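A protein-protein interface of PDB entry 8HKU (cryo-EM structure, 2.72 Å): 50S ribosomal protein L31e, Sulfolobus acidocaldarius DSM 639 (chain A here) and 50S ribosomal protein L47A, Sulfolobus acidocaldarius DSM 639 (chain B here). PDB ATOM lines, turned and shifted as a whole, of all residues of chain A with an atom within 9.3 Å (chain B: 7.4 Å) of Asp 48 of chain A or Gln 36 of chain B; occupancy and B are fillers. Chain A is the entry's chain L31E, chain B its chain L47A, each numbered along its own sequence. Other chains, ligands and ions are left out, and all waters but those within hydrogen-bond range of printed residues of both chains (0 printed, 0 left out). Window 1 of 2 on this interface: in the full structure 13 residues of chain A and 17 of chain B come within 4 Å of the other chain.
Printed residues of chain A that touch a printed residue of chain B: Asp 48, Pro 49, Leu 50 and Lys 72.
Hydrophobic or aromatic side chains of chain A that line the printed part of chain B: Pro 49 and Leu 50.
Hydrophobic or aromatic side chains of chain B that line the printed part of chain A: Leu 19, Ile 34, Phe 35 and Leu 38.
Along chain B the printed residues that touch a printed residue of chain A span positions 19 to 38.
Among the printed residues, 9 pairs touch across the chains.
Among the printed residues, no Asp or Glu carboxylate lies within 4 Å of a Lys or Arg side-chain nitrogen of the other chain.
N of Leu 19 of chain B sits at hydrogen-bond distance from O of Met 12 of chain B (2.8 Å).
The side-chain carboxylate (OD1) of Asp 48 of chain A is in hydrogen-bond range of the backbone NH (N) of Leu 50 of chain A, at 3.0 Å.
The backbone carbonyl oxygen (O) of Leu 38 of chain B is in hydrogen-bond range of the side-chain amide nitrogen (NE2) of Gln 36 of chain B (3.1 Å).
O of Glu 22 of chain B lies within hydrogen-bond range of N of Ile 34 of chain B, 3.2 Å away.
The backbone NH (N) of Leu 20 of chain B sits at hydrogen-bond distance from the backbone carbonyl oxygen (O) of Gln 36 of chain B (2.8 Å).
OD2 of Asp 48 of chain A sits at hydrogen-bond distance from N of Ser 37 of chain B (3.2 Å).
OD2 of Asp 48 of chain A touches CG of Gln 36 of chain B (3.4 Å).
OD2 of Asp 48 of chain A touches CB of Leu 38 of chain B, at 3.5 Å.
Ser 37 of chain B touches Pro 49 of chain A.
CD of Pro 49 of chain A touches CD1 of Leu 38 of chain B, 3.96 Å away.
Leu 19 of chain B touches Leu 50 of chain A.
Leu 50 of chain A touches Phe 35 of chain B (CD1 to CB, 3.97 Å).
Leu 50 of chain A touches Ser 37 of chain B.
Lys 72 of chain A touches Ile 34 of chain B.
Gln 36 of chain B touches just one residue of chain A: Asp 48.
Of chain A, only Asp 48, Pro 49 and Leu 50 come within 4 Å of Ser 37 of chain B.
Of the printed residues of chain B, Lys 72 of chain A touches Ile 34.
Printed residues of chain B within 4 Å of Leu 50 of chain A: Leu 19 (3.6 Å), Phe 35 (3.97 Å) and Ser 37 (3.6 Å).
Of the printed residues of chain A, Leu 19 of chain B touches Leu 50.
The nearest residue of chain B that does not touch Asp 48 of chain A is Phe 35 of chain B (4.7 Å).
The nearest residue of chain A that does not touch Gln 36 of chain B is Lys 72 of chain A (4.3 Å).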
ATOM      1  N   ILE A  29      17.745  -7.949  -2.880  1.00  0.00           N
ATOM      2  CA  ILE A  29      18.381  -7.672  -1.597  1.00  0.00           C
ATOM      3  C   ILE A  29      19.877  -7.469  -1.777  1.00  0.00           C
ATOM      4  O   ILE A  29      20.482  -6.622  -1.112  1.00  0.00           O
ATOM      5  CB  ILE A  29      18.080  -8.799  -0.593  1.00  0.00           C
ATOM      6  CG1 ILE A  29      16.578  -8.945  -0.383  1.00  0.00           C
ATOM      7  CG2 ILE A  29      18.736  -8.522   0.732  1.00  0.00           C
ATOM      8  CD1 ILE A  29      15.956  -7.758   0.276  1.00  0.00           C
ATOM      9  N   VAL A  32      20.696  -3.871  -3.268  1.00  0.00           N
ATOM     10  CA  VAL A  32      20.709  -2.757  -2.331  1.00  0.00           C
ATOM     11  C   VAL A  32      22.038  -2.698  -1.590  1.00  0.00           C
ATOM     12  O   VAL A  32      22.554  -1.614  -1.306  1.00  0.00           O
ATOM     13  CB  VAL A  32      19.513  -2.868  -1.371  1.00  0.00           C
ATOM     14  CG1 VAL A  32      19.628  -1.875  -0.248  1.00  0.00           C
ATOM     15  CG2 VAL A  32      18.226  -2.638  -2.123  1.00  0.00           C
ATOM     16  N   ARG A  33      22.615  -3.853  -1.266  1.00  0.00           N
ATOM     17  CA  ARG A  33      23.920  -3.858  -0.615  1.00  0.00           C
ATOM     18  C   ARG A  33      24.993  -3.307  -1.533  1.00  0.00           C
ATOM     19  O   ARG A  33      25.892  -2.590  -1.087  1.00  0.00           O
ATOM     20  CB  ARG A  33      24.292  -5.267  -0.179  1.00  0.00           C
ATOM     21  CG  ARG A  33      23.543  -5.747   1.012  1.00  0.00           C
ATOM     22  CD  ARG A  33      24.082  -7.063   1.493  1.00  0.00           C
ATOM     23  NE  ARG A  33      23.679  -7.329   2.867  1.00  0.00           N
ATOM     24  CZ  ARG A  33      22.670  -8.113   3.213  1.00  0.00           C
ATOM     25  NH1 ARG A  33      21.926  -8.722   2.310  1.00  0.00           N
ATOM     26  NH2 ARG A  33      22.397  -8.284   4.500  1.00  0.00           N
ATOM     27  N   VAL A  45      26.897  -3.457   5.265  1.00  0.00           N
ATOM     28  CA  VAL A  45      25.583  -2.861   5.083  1.00  0.00           C
ATOM     29  C   VAL A  45      24.572  -3.663   5.884  1.00  0.00           C
ATOM     30  O   VAL A  45      24.572  -4.896   5.834  1.00  0.00           O
ATOM     31  CB  VAL A  45      25.184  -2.811   3.600  1.00  0.00           C
ATOM     32  CG1 VAL A  45      23.828  -2.180   3.445  1.00  0.00           C
ATOM     33  CG2 VAL A  45      26.213  -2.046   2.814  1.00  0.00           C
ATOM     34  N   ILE A  46      23.716  -2.965   6.618  1.00  0.00           N
ATOM     35  CA  ILE A  46      22.638  -3.573   7.383  1.00  0.00           C
ATOM     36  C   ILE A  46      21.321  -3.115   6.779  1.00  0.00           C
ATOM     37  O   ILE A  46      21.098  -1.914   6.610  1.00  0.00           O
ATOM     38  CB  ILE A  46      22.730  -3.200   8.870  1.00  0.00           C
ATOM     39  CG1 ILE A  46      24.023  -3.749   9.461  1.00  0.00           C
ATOM     40  CG2 ILE A  46      21.535  -3.714   9.622  1.00  0.00           C
ATOM     41  CD1 ILE A  46      24.124  -3.601  10.936  1.00  0.00           C
ATOM     42  N   ILE A  47      20.460  -4.067   6.437  1.00  0.00           N
ATOM     43  CA  ILE A  47      19.145  -3.776   5.881  1.00  0.00           C
ATOM     44  C   ILE A  47      18.102  -3.873   6.979  1.00  0.00           C
ATOM     45  O   ILE A  47      17.995  -4.897   7.660  1.00  0.00           O
ATOM     46  CB  ILE A  47      18.798  -4.709   4.709  1.00  0.00           C
ATOM     47  CG1 ILE A  47      19.758  -4.509   3.539  1.00  0.00           C
ATOM     48  CG2 ILE A  47      17.383  -4.491   4.265  1.00  0.00           C
ATOM     49  CD1 ILE A  47      21.011  -5.285   3.610  1.00  0.00           C
ATOM     50  N   ASP A  48      17.342  -2.805   7.153  1.00  0.00           N
ATOM     51  CA  ASP A  48      16.254  -2.810   8.112  1.00  0.00           C
ATOM     52  C   ASP A  48      15.216  -3.851   7.707  1.00  0.00           C
ATOM     53  O   ASP A  48      14.876  -3.954   6.524  1.00  0.00           O
ATOM     54  CB  ASP A  48      15.616  -1.425   8.174  1.00  0.00           C
ATOM     55  CG  ASP A  48      14.765  -1.234   9.395  1.00  0.00           C
ATOM     56  OD1 ASP A  48      13.633  -1.754   9.420  1.00  0.00           O
ATOM     57  OD2 ASP A  48      15.229  -0.564  10.336  1.00  0.00           O
ATOM     58  N   PRO A  49      14.693  -4.636   8.651  1.00  0.00           N
ATOM     59  CA  PRO A  49      13.704  -5.657   8.281  1.00  0.00           C
ATOM     60  C   PRO A  49      12.471  -5.093   7.609  1.00  0.00           C
ATOM     61  O   PRO A  49      11.834  -5.799   6.822  1.00  0.00           O
ATOM     62  CB  PRO A  49      13.369  -6.310   9.624  1.00  0.00           C
ATOM     63  CG  PRO A  49      14.569  -6.094  10.441  1.00  0.00           C
ATOM     64  CD  PRO A  49      15.090  -4.752  10.061  1.00  0.00           C
ATOM     65  N   LEU A  50      12.105  -3.846   7.897  1.00  0.00           N
ATOM     66  CA  LEU A  50      10.969  -3.237   7.218  1.00  0.00           C
ATOM     67  C   LEU A  50      11.257  -2.999   5.744  1.00  0.00           C
ATOM     68  O   LEU A  50      10.363  -3.137   4.906  1.00  0.00           O
ATOM     69  CB  LEU A  50      10.594  -1.924   7.895  1.00  0.00           C
ATOM     70  CG  LEU A  50       9.488  -1.983   8.934  1.00  0.00           C
ATOM     71  CD1 LEU A  50       9.098  -0.586   9.320  1.00  0.00           C
ATOM     72  CD2 LEU A  50       8.308  -2.728   8.374  1.00  0.00           C
ATOM     73  N   LEU A  51      12.485  -2.601   5.414  1.00  0.00           N
ATOM     74  CA  LEU A  51      12.834  -2.352   4.021  1.00  0.00           C
ATOM     75  C   LEU A  51      12.786  -3.633   3.205  1.00  0.00           C
ATOM     76  O   LEU A  51      12.285  -3.640   2.079  1.00  0.00           O
ATOM     77  CB  LEU A  51      14.217  -1.711   3.936  1.00  0.00           C
ATOM     78  CG  LEU A  51      14.871  -1.565   2.565  1.00  0.00           C
ATOM     79  CD1 LEU A  51      14.114  -0.607   1.701  1.00  0.00           C
ATOM     80  CD2 LEU A  51      16.289  -1.116   2.721  1.00  0.00           C
ATOM     81  N   ALA A  52      13.286  -4.732   3.767  1.00  0.00           N
ATOM     82  CA  ALA A  52      13.328  -5.991   3.037  1.00  0.00           C
ATOM     83  C   ALA A  52      11.933  -6.478   2.674  1.00  0.00           C
ATOM     84  O   ALA A  52      11.743  -7.100   1.627  1.00  0.00           O
ATOM     85  CB  ALA A  52      14.069  -7.039   3.857  1.00  0.00           C
ATOM     86  N   LYS A  53      10.948  -6.233   3.532  1.00  0.00           N
ATOM     87  CA  LYS A  53       9.579  -6.616   3.218  1.00  0.00           C
ATOM     88  C   LYS A  53       8.900  -5.660   2.249  1.00  0.00           C
ATOM     89  O   LYS A  53       7.911  -6.042   1.620  1.00  0.00           O
ATOM     90  CB  LYS A  53       8.757  -6.717   4.500  1.00  0.00           C
ATOM     91  CG  LYS A  53       9.363  -7.653   5.523  1.00  0.00           C
ATOM     92  CD  LYS A  53       8.724  -7.512   6.894  1.00  0.00           C
ATOM     93  CE  LYS A  53       9.464  -8.351   7.920  1.00  0.00           C
ATOM     94  NZ  LYS A  53       9.094  -7.978   9.303  1.00  0.00           N
ATOM     95  N   ALA A  54       9.382  -4.424   2.139  1.00  0.00           N
ATOM     96  CA  ALA A  54       8.803  -3.471   1.203  1.00  0.00           C
ATOM     97  C   ALA A  54       9.258  -3.719  -0.227  1.00  0.00           C
ATOM     98  O   ALA A  54       8.497  -3.468  -1.165  1.00  0.00           O
ATOM     99  CB  ALA A  54       9.156  -2.047   1.621  1.00  0.00           C
ATOM    100  N   ILE A  55      10.490  -4.190  -0.411  1.00  0.00           N
ATOM    101  CA  ILE A  55      10.987  -4.506  -1.745  1.00  0.00           C
ATOM    102  C   ILE A  55      10.137  -5.590  -2.383  1.00  0.00           C
ATOM    103  O   ILE A  55       9.797  -5.522  -3.568  1.00  0.00           O
ATOM    104  CB  ILE A  55      12.461  -4.931  -1.674  1.00  0.00           C
ATOM    105  CG1 ILE A  55      13.330  -3.794  -1.162  1.00  0.00           C
ATOM    106  CG2 ILE A  55      12.945  -5.395  -3.025  1.00  0.00           C
ATOM    107  CD1 ILE A  55      14.774  -4.178  -1.028  1.00  0.00           C
ATOM    108  N   ILE A  69      15.226   4.883  -0.404  1.00  0.00           N
ATOM    109  CA  ILE A  69      15.782   4.486   0.879  1.00  0.00           C
ATOM    110  C   ILE A  69      16.475   5.680   1.512  1.00  0.00           C
ATOM    111  O   ILE A  69      16.799   6.663   0.849  1.00  0.00           O
ATOM    112  CB  ILE A  69      16.770   3.312   0.760  1.00  0.00           C
ATOM    113  CG1 ILE A  69      17.963   3.710  -0.093  1.00  0.00           C
ATOM    114  CG2 ILE A  69      16.105   2.122   0.140  1.00  0.00           C
ATOM    115  CD1 ILE A  69      19.142   2.823   0.098  1.00  0.00           C
ATOM    116  N   ALA A  70      16.700   5.580   2.819  1.00  0.00           N
ATOM    117  CA  ALA A  70      17.450   6.569   3.578  1.00  0.00           C
ATOM    118  C   ALA A  70      18.537   5.855   4.358  1.00  0.00           C
ATOM    119  O   ALA A  70      18.246   4.933   5.120  1.00  0.00           O
ATOM    120  CB  ALA A  70      16.544   7.342   4.529  1.00  0.00           C
ATOM    121  N   VAL A  71      19.777   6.285   4.186  1.00  0.00           N
ATOM    122  CA  VAL A  71      20.928   5.604   4.761  1.00  0.00           C
ATOM    123  C   VAL A  71      21.450   6.451   5.909  1.00  0.00           C
ATOM    124  O   VAL A  71      21.894   7.584   5.705  1.00  0.00           O
ATOM    125  CB  VAL A  71      22.024   5.358   3.718  1.00  0.00           C
ATOM    126  CG1 VAL A  71      23.134   4.530   4.307  1.00  0.00           C
ATOM    127  CG2 VAL A  71      21.449   4.678   2.501  1.00  0.00           C
ATOM    128  N   LYS A  72      21.392   5.908   7.120  1.00  0.00           N
ATOM    129  CA  LYS A  72      22.008   6.532   8.289  1.00  0.00           C
ATOM    130  C   LYS A  72      23.417   5.969   8.435  1.00  0.00           C
ATOM    131  O   LYS A  72      23.726   5.179   9.321  1.00  0.00           O
ATOM    132  CB  LYS A  72      21.172   6.282   9.538  1.00  0.00           C
ATOM    133  CG  LYS A  72      20.021   7.258   9.755  1.00  0.00           C
ATOM    134  CD  LYS A  72      18.820   6.950   8.857  1.00  0.00           C
ATOM    135  CE  LYS A  72      18.126   5.666   9.272  1.00  0.00           C
ATOM    136  NZ  LYS A  72      16.929   5.376   8.448  1.00  0.00           N
ATOM    137  N   ILE A  74      26.335   5.504   9.623  1.00  0.00           N
ATOM    138  CA  ILE A  74      27.151   5.807  10.787  1.00  0.00           C
ATOM    139  C   ILE A  74      28.569   5.297  10.552  1.00  0.00           C
ATOM    140  O   ILE A  74      28.834   4.603   9.565  1.00  0.00           O
ATOM    141  CB  ILE A  74      26.532   5.194  12.051  1.00  0.00           C
ATOM    142  CG1 ILE A  74      26.386   3.687  11.891  1.00  0.00           C
ATOM    143  CG2 ILE A  74      25.173   5.796  12.308  1.00  0.00           C
ATOM    144  CD1 ILE A  74      27.209   2.920  12.860  1.00  0.00           C
ATOM    145  N   LYS B   9      10.107  13.093  15.680  1.00  0.00           N
ATOM    146  CA  LYS B   9      10.436  11.687  15.858  1.00  0.00           C
ATOM    147  C   LYS B   9       9.442  11.061  16.823  1.00  0.00           C
ATOM    148  O   LYS B   9       9.129  11.643  17.865  1.00  0.00           O
ATOM    149  CB  LYS B   9      11.860  11.515  16.385  1.00  0.00           C
ATOM    150  CG  LYS B   9      12.314  10.077  16.494  1.00  0.00           C
ATOM    151  CD  LYS B   9      13.749   9.998  16.963  1.00  0.00           C
ATOM    152  CE  LYS B   9      14.673  10.699  15.987  1.00  0.00           C
ATOM    153  NZ  LYS B   9      16.065  10.778  16.500  1.00  0.00           N
ATOM    154  N   TYR B  10       8.952   9.874  16.480  1.00  0.00           N
ATOM    155  CA  TYR B  10       7.911   9.206  17.246  1.00  0.00           C
ATOM    156  C   TYR B  10       8.372   7.808  17.640  1.00  0.00           C
ATOM    157  O   TYR B  10       9.461   7.359  17.276  1.00  0.00           O
ATOM    158  CB  TYR B  10       6.604   9.137  16.451  1.00  0.00           C
ATOM    159  CG  TYR B  10       6.043  10.491  16.103  1.00  0.00           C
ATOM    160  CD1 TYR B  10       5.388  11.255  17.056  1.00  0.00           C
ATOM    161  CD2 TYR B  10       6.175  11.008  14.826  1.00  0.00           C
ATOM    162  CE1 TYR B  10       4.875  12.492  16.744  1.00  0.00           C
ATOM    163  CE2 TYR B  10       5.664  12.247  14.505  1.00  0.00           C
ATOM    164  CZ  TYR B  10       5.014  12.983  15.468  1.00  0.00           C
ATOM    165  OH  TYR B  10       4.504  14.219  15.154  1.00  0.00           O
ATOM    166  N   MET B  12       6.160   4.039  18.275  1.00  0.00           N
ATOM    167  CA  MET B  12       4.881   3.352  18.333  1.00  0.00           C
ATOM    168  C   MET B  12       5.120   1.850  18.390  1.00  0.00           C
ATOM    169  O   MET B  12       6.100   1.344  17.841  1.00  0.00           O
ATOM    170  CB  MET B  12       4.009   3.722  17.125  1.00  0.00           C
ATOM    171  CG  MET B  12       2.628   3.100  17.113  1.00  0.00           C
ATOM    172  SD  MET B  12       1.665   3.612  15.679  1.00  0.00           S
ATOM    173  CE  MET B  12       2.497   2.720  14.374  1.00  0.00           C
ATOM    174  N   GLU B  18       8.444  -2.829  17.997  1.00  0.00           N
ATOM    175  CA  GLU B  18       8.749  -1.417  18.175  1.00  0.00           C
ATOM    176  C   GLU B  18       9.009  -0.740  16.835  1.00  0.00           C
ATOM    177  O   GLU B  18       9.689  -1.296  15.968  1.00  0.00           O
ATOM    178  CB  GLU B  18       9.964  -1.244  19.091  1.00  0.00           C
ATOM    179  CG  GLU B  18      10.514   0.184  19.222  1.00  0.00           C
ATOM    180  CD  GLU B  18       9.542   1.200  19.822  1.00  0.00           C
ATOM    181  OE1 GLU B  18       8.311   0.993  19.799  1.00  0.00           O
ATOM    182  OE2 GLU B  18      10.031   2.225  20.341  1.00  0.00           O
ATOM    183  N   LEU B  19       8.462   0.465  16.675  1.00  0.00           N
ATOM    184  CA  LEU B  19       8.654   1.285  15.487  1.00  0.00           C
ATOM    185  C   LEU B  19       9.239   2.643  15.843  1.00  0.00           C
ATOM    186  O   LEU B  19       8.992   3.186  16.922  1.00  0.00           O
ATOM    187  CB  LEU B  19       7.345   1.510  14.727  1.00  0.00           C
ATOM    188  CG  LEU B  19       7.066   0.626  13.520  1.00  0.00           C
ATOM    189  CD1 LEU B  19       5.771   1.045  12.859  1.00  0.00           C
ATOM    190  CD2 LEU B  19       8.214   0.738  12.548  1.00  0.00           C
ATOM    191  N   LEU B  20      10.020   3.184  14.913  1.00  0.00           N
ATOM    192  CA  LEU B  20      10.486   4.561  14.957  1.00  0.00           C
ATOM    193  C   LEU B  20      10.095   5.244  13.658  1.00  0.00           C
ATOM    194  O   LEU B  20      10.414   4.747  12.575  1.00  0.00           O
ATOM    195  CB  LEU B  20      12.000   4.636  15.152  1.00  0.00           C
ATOM    196  CG  LEU B  20      12.549   4.273  16.528  1.00  0.00           C
ATOM    197  CD1 LEU B  20      14.063   4.246  16.494  1.00  0.00           C
ATOM    198  CD2 LEU B  20      12.050   5.250  17.572  1.00  0.00           C
ATOM    199  N   ILE B  21       9.407   6.376  13.763  1.00  0.00           N
ATOM    200  CA  ILE B  21       9.006   7.169  12.608  1.00  0.00           C
ATOM    201  C   ILE B  21       9.637   8.546  12.737  1.00  0.00           C
ATOM    202  O   ILE B  21       9.540   9.181  13.792  1.00  0.00           O
ATOM    203  CB  ILE B  21       7.477   7.283  12.491  1.00  0.00           C
ATOM    204  CG1 ILE B  21       6.848   5.896  12.385  1.00  0.00           C
ATOM    205  CG2 ILE B  21       7.102   8.127  11.292  1.00  0.00           C
ATOM    206  CD1 ILE B  21       5.354   5.925  12.184  1.00  0.00           C
ATOM    207  N   GLU B  22      10.288   8.999  11.672  1.00  0.00           N
ATOM    208  CA  GLU B  22      10.940  10.297  11.644  1.00  0.00           C
ATOM    209  C   GLU B  22      10.379  11.130  10.503  1.00  0.00           C
ATOM    210  O   GLU B  22      10.140  10.616   9.406  1.00  0.00           O
ATOM    211  CB  GLU B  22      12.453  10.154  11.488  1.00  0.00           C
ATOM    212  CG  GLU B  22      13.138   9.573  12.704  1.00  0.00           C
ATOM    213  CD  GLU B  22      14.569   9.171  12.428  1.00  0.00           C
ATOM    214  OE1 GLU B  22      15.198   9.788  11.544  1.00  0.00           O
ATOM    215  OE2 GLU B  22      15.063   8.235  13.091  1.00  0.00           O
ATOM    216  N   ILE B  34      10.527   8.418   7.180  1.00  0.00           N
ATOM    217  CA  ILE B  34      11.514   7.352   7.306  1.00  0.00           C
ATOM    218  C   ILE B  34      11.019   6.361   8.351  1.00  0.00           C
ATOM    219  O   ILE B  34      10.754   6.739   9.498  1.00  0.00           O
ATOM    220  CB  ILE B  34      12.894   7.907   7.680  1.00  0.00           C
ATOM    221  CG1 ILE B  34      13.321   8.966   6.668  1.00  0.00           C
ATOM    222  CG2 ILE B  34      13.915   6.792   7.739  1.00  0.00           C
ATOM    223  CD1 ILE B  34      14.516   9.769   7.097  1.00  0.00           C
ATOM    224  N   PHE B  35      10.907   5.093   7.959  1.00  0.00           N
ATOM    225  CA  PHE B  35      10.416   4.028   8.825  1.00  0.00           C
ATOM    226  C   PHE B  35      11.586   3.150   9.242  1.00  0.00           C
ATOM    227  O   PHE B  35      12.276   2.589   8.388  1.00  0.00           O
ATOM    228  CB  PHE B  35       9.358   3.185   8.117  1.00  0.00           C
ATOM    229  CG  PHE B  35       8.133   3.950   7.725  1.00  0.00           C
ATOM    230  CD1 PHE B  35       7.079   4.093   8.607  1.00  0.00           C
ATOM    231  CD2 PHE B  35       8.028   4.512   6.466  1.00  0.00           C
ATOM    232  CE1 PHE B  35       5.949   4.793   8.245  1.00  0.00           C
ATOM    233  CE2 PHE B  35       6.899   5.210   6.098  1.00  0.00           C
ATOM    234  CZ  PHE B  35       5.859   5.351   6.991  1.00  0.00           C
ATOM    235  N   GLN B  36      11.793   3.017  10.547  1.00  0.00           N
ATOM    236  CA  GLN B  36      12.859   2.186  11.087  1.00  0.00           C
ATOM    237  C   GLN B  36      12.289   1.253  12.141  1.00  0.00           C
ATOM    238  O   GLN B  36      11.604   1.703  13.064  1.00  0.00           O
ATOM    239  CB  GLN B  36      13.969   3.040  11.697  1.00  0.00           C
ATOM    240  CG  GLN B  36      15.125   2.242  12.258  1.00  0.00           C
ATOM    241  CD  GLN B  36      16.231   3.125  12.795  1.00  0.00           C
ATOM    242  OE1 GLN B  36      16.102   4.346  12.824  1.00  0.00           O
ATOM    243  NE2 GLN B  36      17.322   2.512  13.229  1.00  0.00           N
ATOM    244  N   SER B  37      12.566  -0.040  12.006  1.00  0.00           N
ATOM    245  CA  SER B  37      12.269  -1.000  13.062  1.00  0.00           C
ATOM    246  C   SER B  37      13.534  -1.790  13.335  1.00  0.00           C
ATOM    247  O   SER B  37      13.657  -2.941  12.911  1.00  0.00           O
ATOM    248  CB  SER B  37      11.132  -1.938  12.659  1.00  0.00           C
ATOM    249  OG  SER B  37      11.583  -2.897  11.720  1.00  0.00           O
ATOM    250  N   LEU B  38      14.451  -1.172  14.069  1.00  0.00           N
ATOM    251  CA  LEU B  38      15.716  -1.775  14.455  1.00  0.00           C
ATOM    252  C   LEU B  38      16.366  -0.863  15.484  1.00  0.00           C
ATOM    253  O   LEU B  38      16.489   0.343  15.254  1.00  0.00           O
ATOM    254  CB  LEU B  38      16.618  -1.981  13.232  1.00  0.00           C
ATOM    255  CG  LEU B  38      17.939  -2.727  13.429  1.00  0.00           C
ATOM    256  CD1 LEU B  38      18.190  -3.682  12.284  1.00  0.00           C
ATOM    257  CD2 LEU B  38      19.087  -1.744  13.543  1.00  0.00           C
ATOM    258  N   THR B  39      16.778  -1.414  16.620  1.00  0.00           N
ATOM    259  CA  THR B  39      17.356  -0.597  17.676  1.00  0.00           C
ATOM    260  C   THR B  39      18.815  -0.918  17.947  1.00  0.00           C
ATOM    261  O   THR B  39      19.589  -0.012  18.267  1.00  0.00           O
ATOM    262  CB  THR B  39      16.554  -0.761  18.972  1.00  0.00           C
ATOM    263  OG1 THR B  39      15.156  -0.628  18.686  1.00  0.00           O
ATOM    264  CG2 THR B  39      16.951   0.301  19.985  1.00  0.00           C
ATOM    265  N   SER B  40      19.212  -2.177  17.815  1.00  0.00           N
ATOM    266  CA  SER B  40      20.575  -2.597  18.085  1.00  0.00           C
ATOM    267  C   SER B  40      21.068  -3.495  16.964  1.00  0.00           C
ATOM    268  O   SER B  40      20.301  -4.271  16.386  1.00  0.00           O
ATOM    269  CB  SER B  40      20.670  -3.326  19.427  1.00  0.00           C
ATOM    270  OG  SER B  40      19.809  -4.449  19.460  1.00  0.00           O
ATOM    271  N   TRP B  49      26.064  -1.357  18.536  1.00  0.00           N
ATOM    272  CA  TRP B  49      25.492  -0.034  18.339  1.00  0.00           C
ATOM    273  C   TRP B  49      24.051  -0.032  18.827  1.00  0.00           C
ATOM    274  O   TRP B  49      23.312  -0.993  18.600  1.00  0.00           O
ATOM    275  CB  TRP B  49      25.549   0.386  16.867  1.00  0.00           C
ATOM    276  CG  TRP B  49      24.732   1.602  16.568  1.00  0.00           C
ATOM    277  CD1 TRP B  49      25.101   2.898  16.759  1.00  0.00           C
ATOM    278  CD2 TRP B  49      23.408   1.638  16.025  1.00  0.00           C
ATOM    279  NE1 TRP B  49      24.089   3.741  16.373  1.00  0.00           N
ATOM    280  CE2 TRP B  49      23.038   2.991  15.918  1.00  0.00           C
ATOM    281  CE3 TRP B  49      22.499   0.657  15.621  1.00  0.00           C
ATOM    282  CZ2 TRP B  49      21.802   3.388  15.424  1.00  0.00           C
ATOM    283  CZ3 TRP B  49      21.272   1.054  15.131  1.00  0.00           C
ATOM    284  CH2 TRP B  49      20.934   2.407  15.037  1.00  0.00           C
ATOM    285  N   GLU B  51      20.526   2.441  19.003  1.00  0.00           N
ATOM    286  CA  GLU B  51      19.803   3.651  18.641  1.00  0.00           C
ATOM    287  C   GLU B  51      19.371   4.403  19.893  1.00  0.00           C
ATOM    288  O   GLU B  51      18.947   3.802  20.884  1.00  0.00           O
ATOM    289  CB  GLU B  51      18.583   3.298  17.791  1.00  0.00           C
ATOM    290  CG  GLU B  51      17.654   4.461  17.482  1.00  0.00           C
ATOM    291  CD  GLU B  51      18.225   5.420  16.456  1.00  0.00           C
ATOM    292  OE1 GLU B  51      19.034   4.982  15.612  1.00  0.00           O
ATOM    293  OE2 GLU B  51      17.860   6.613  16.486  1.00  0.00           O
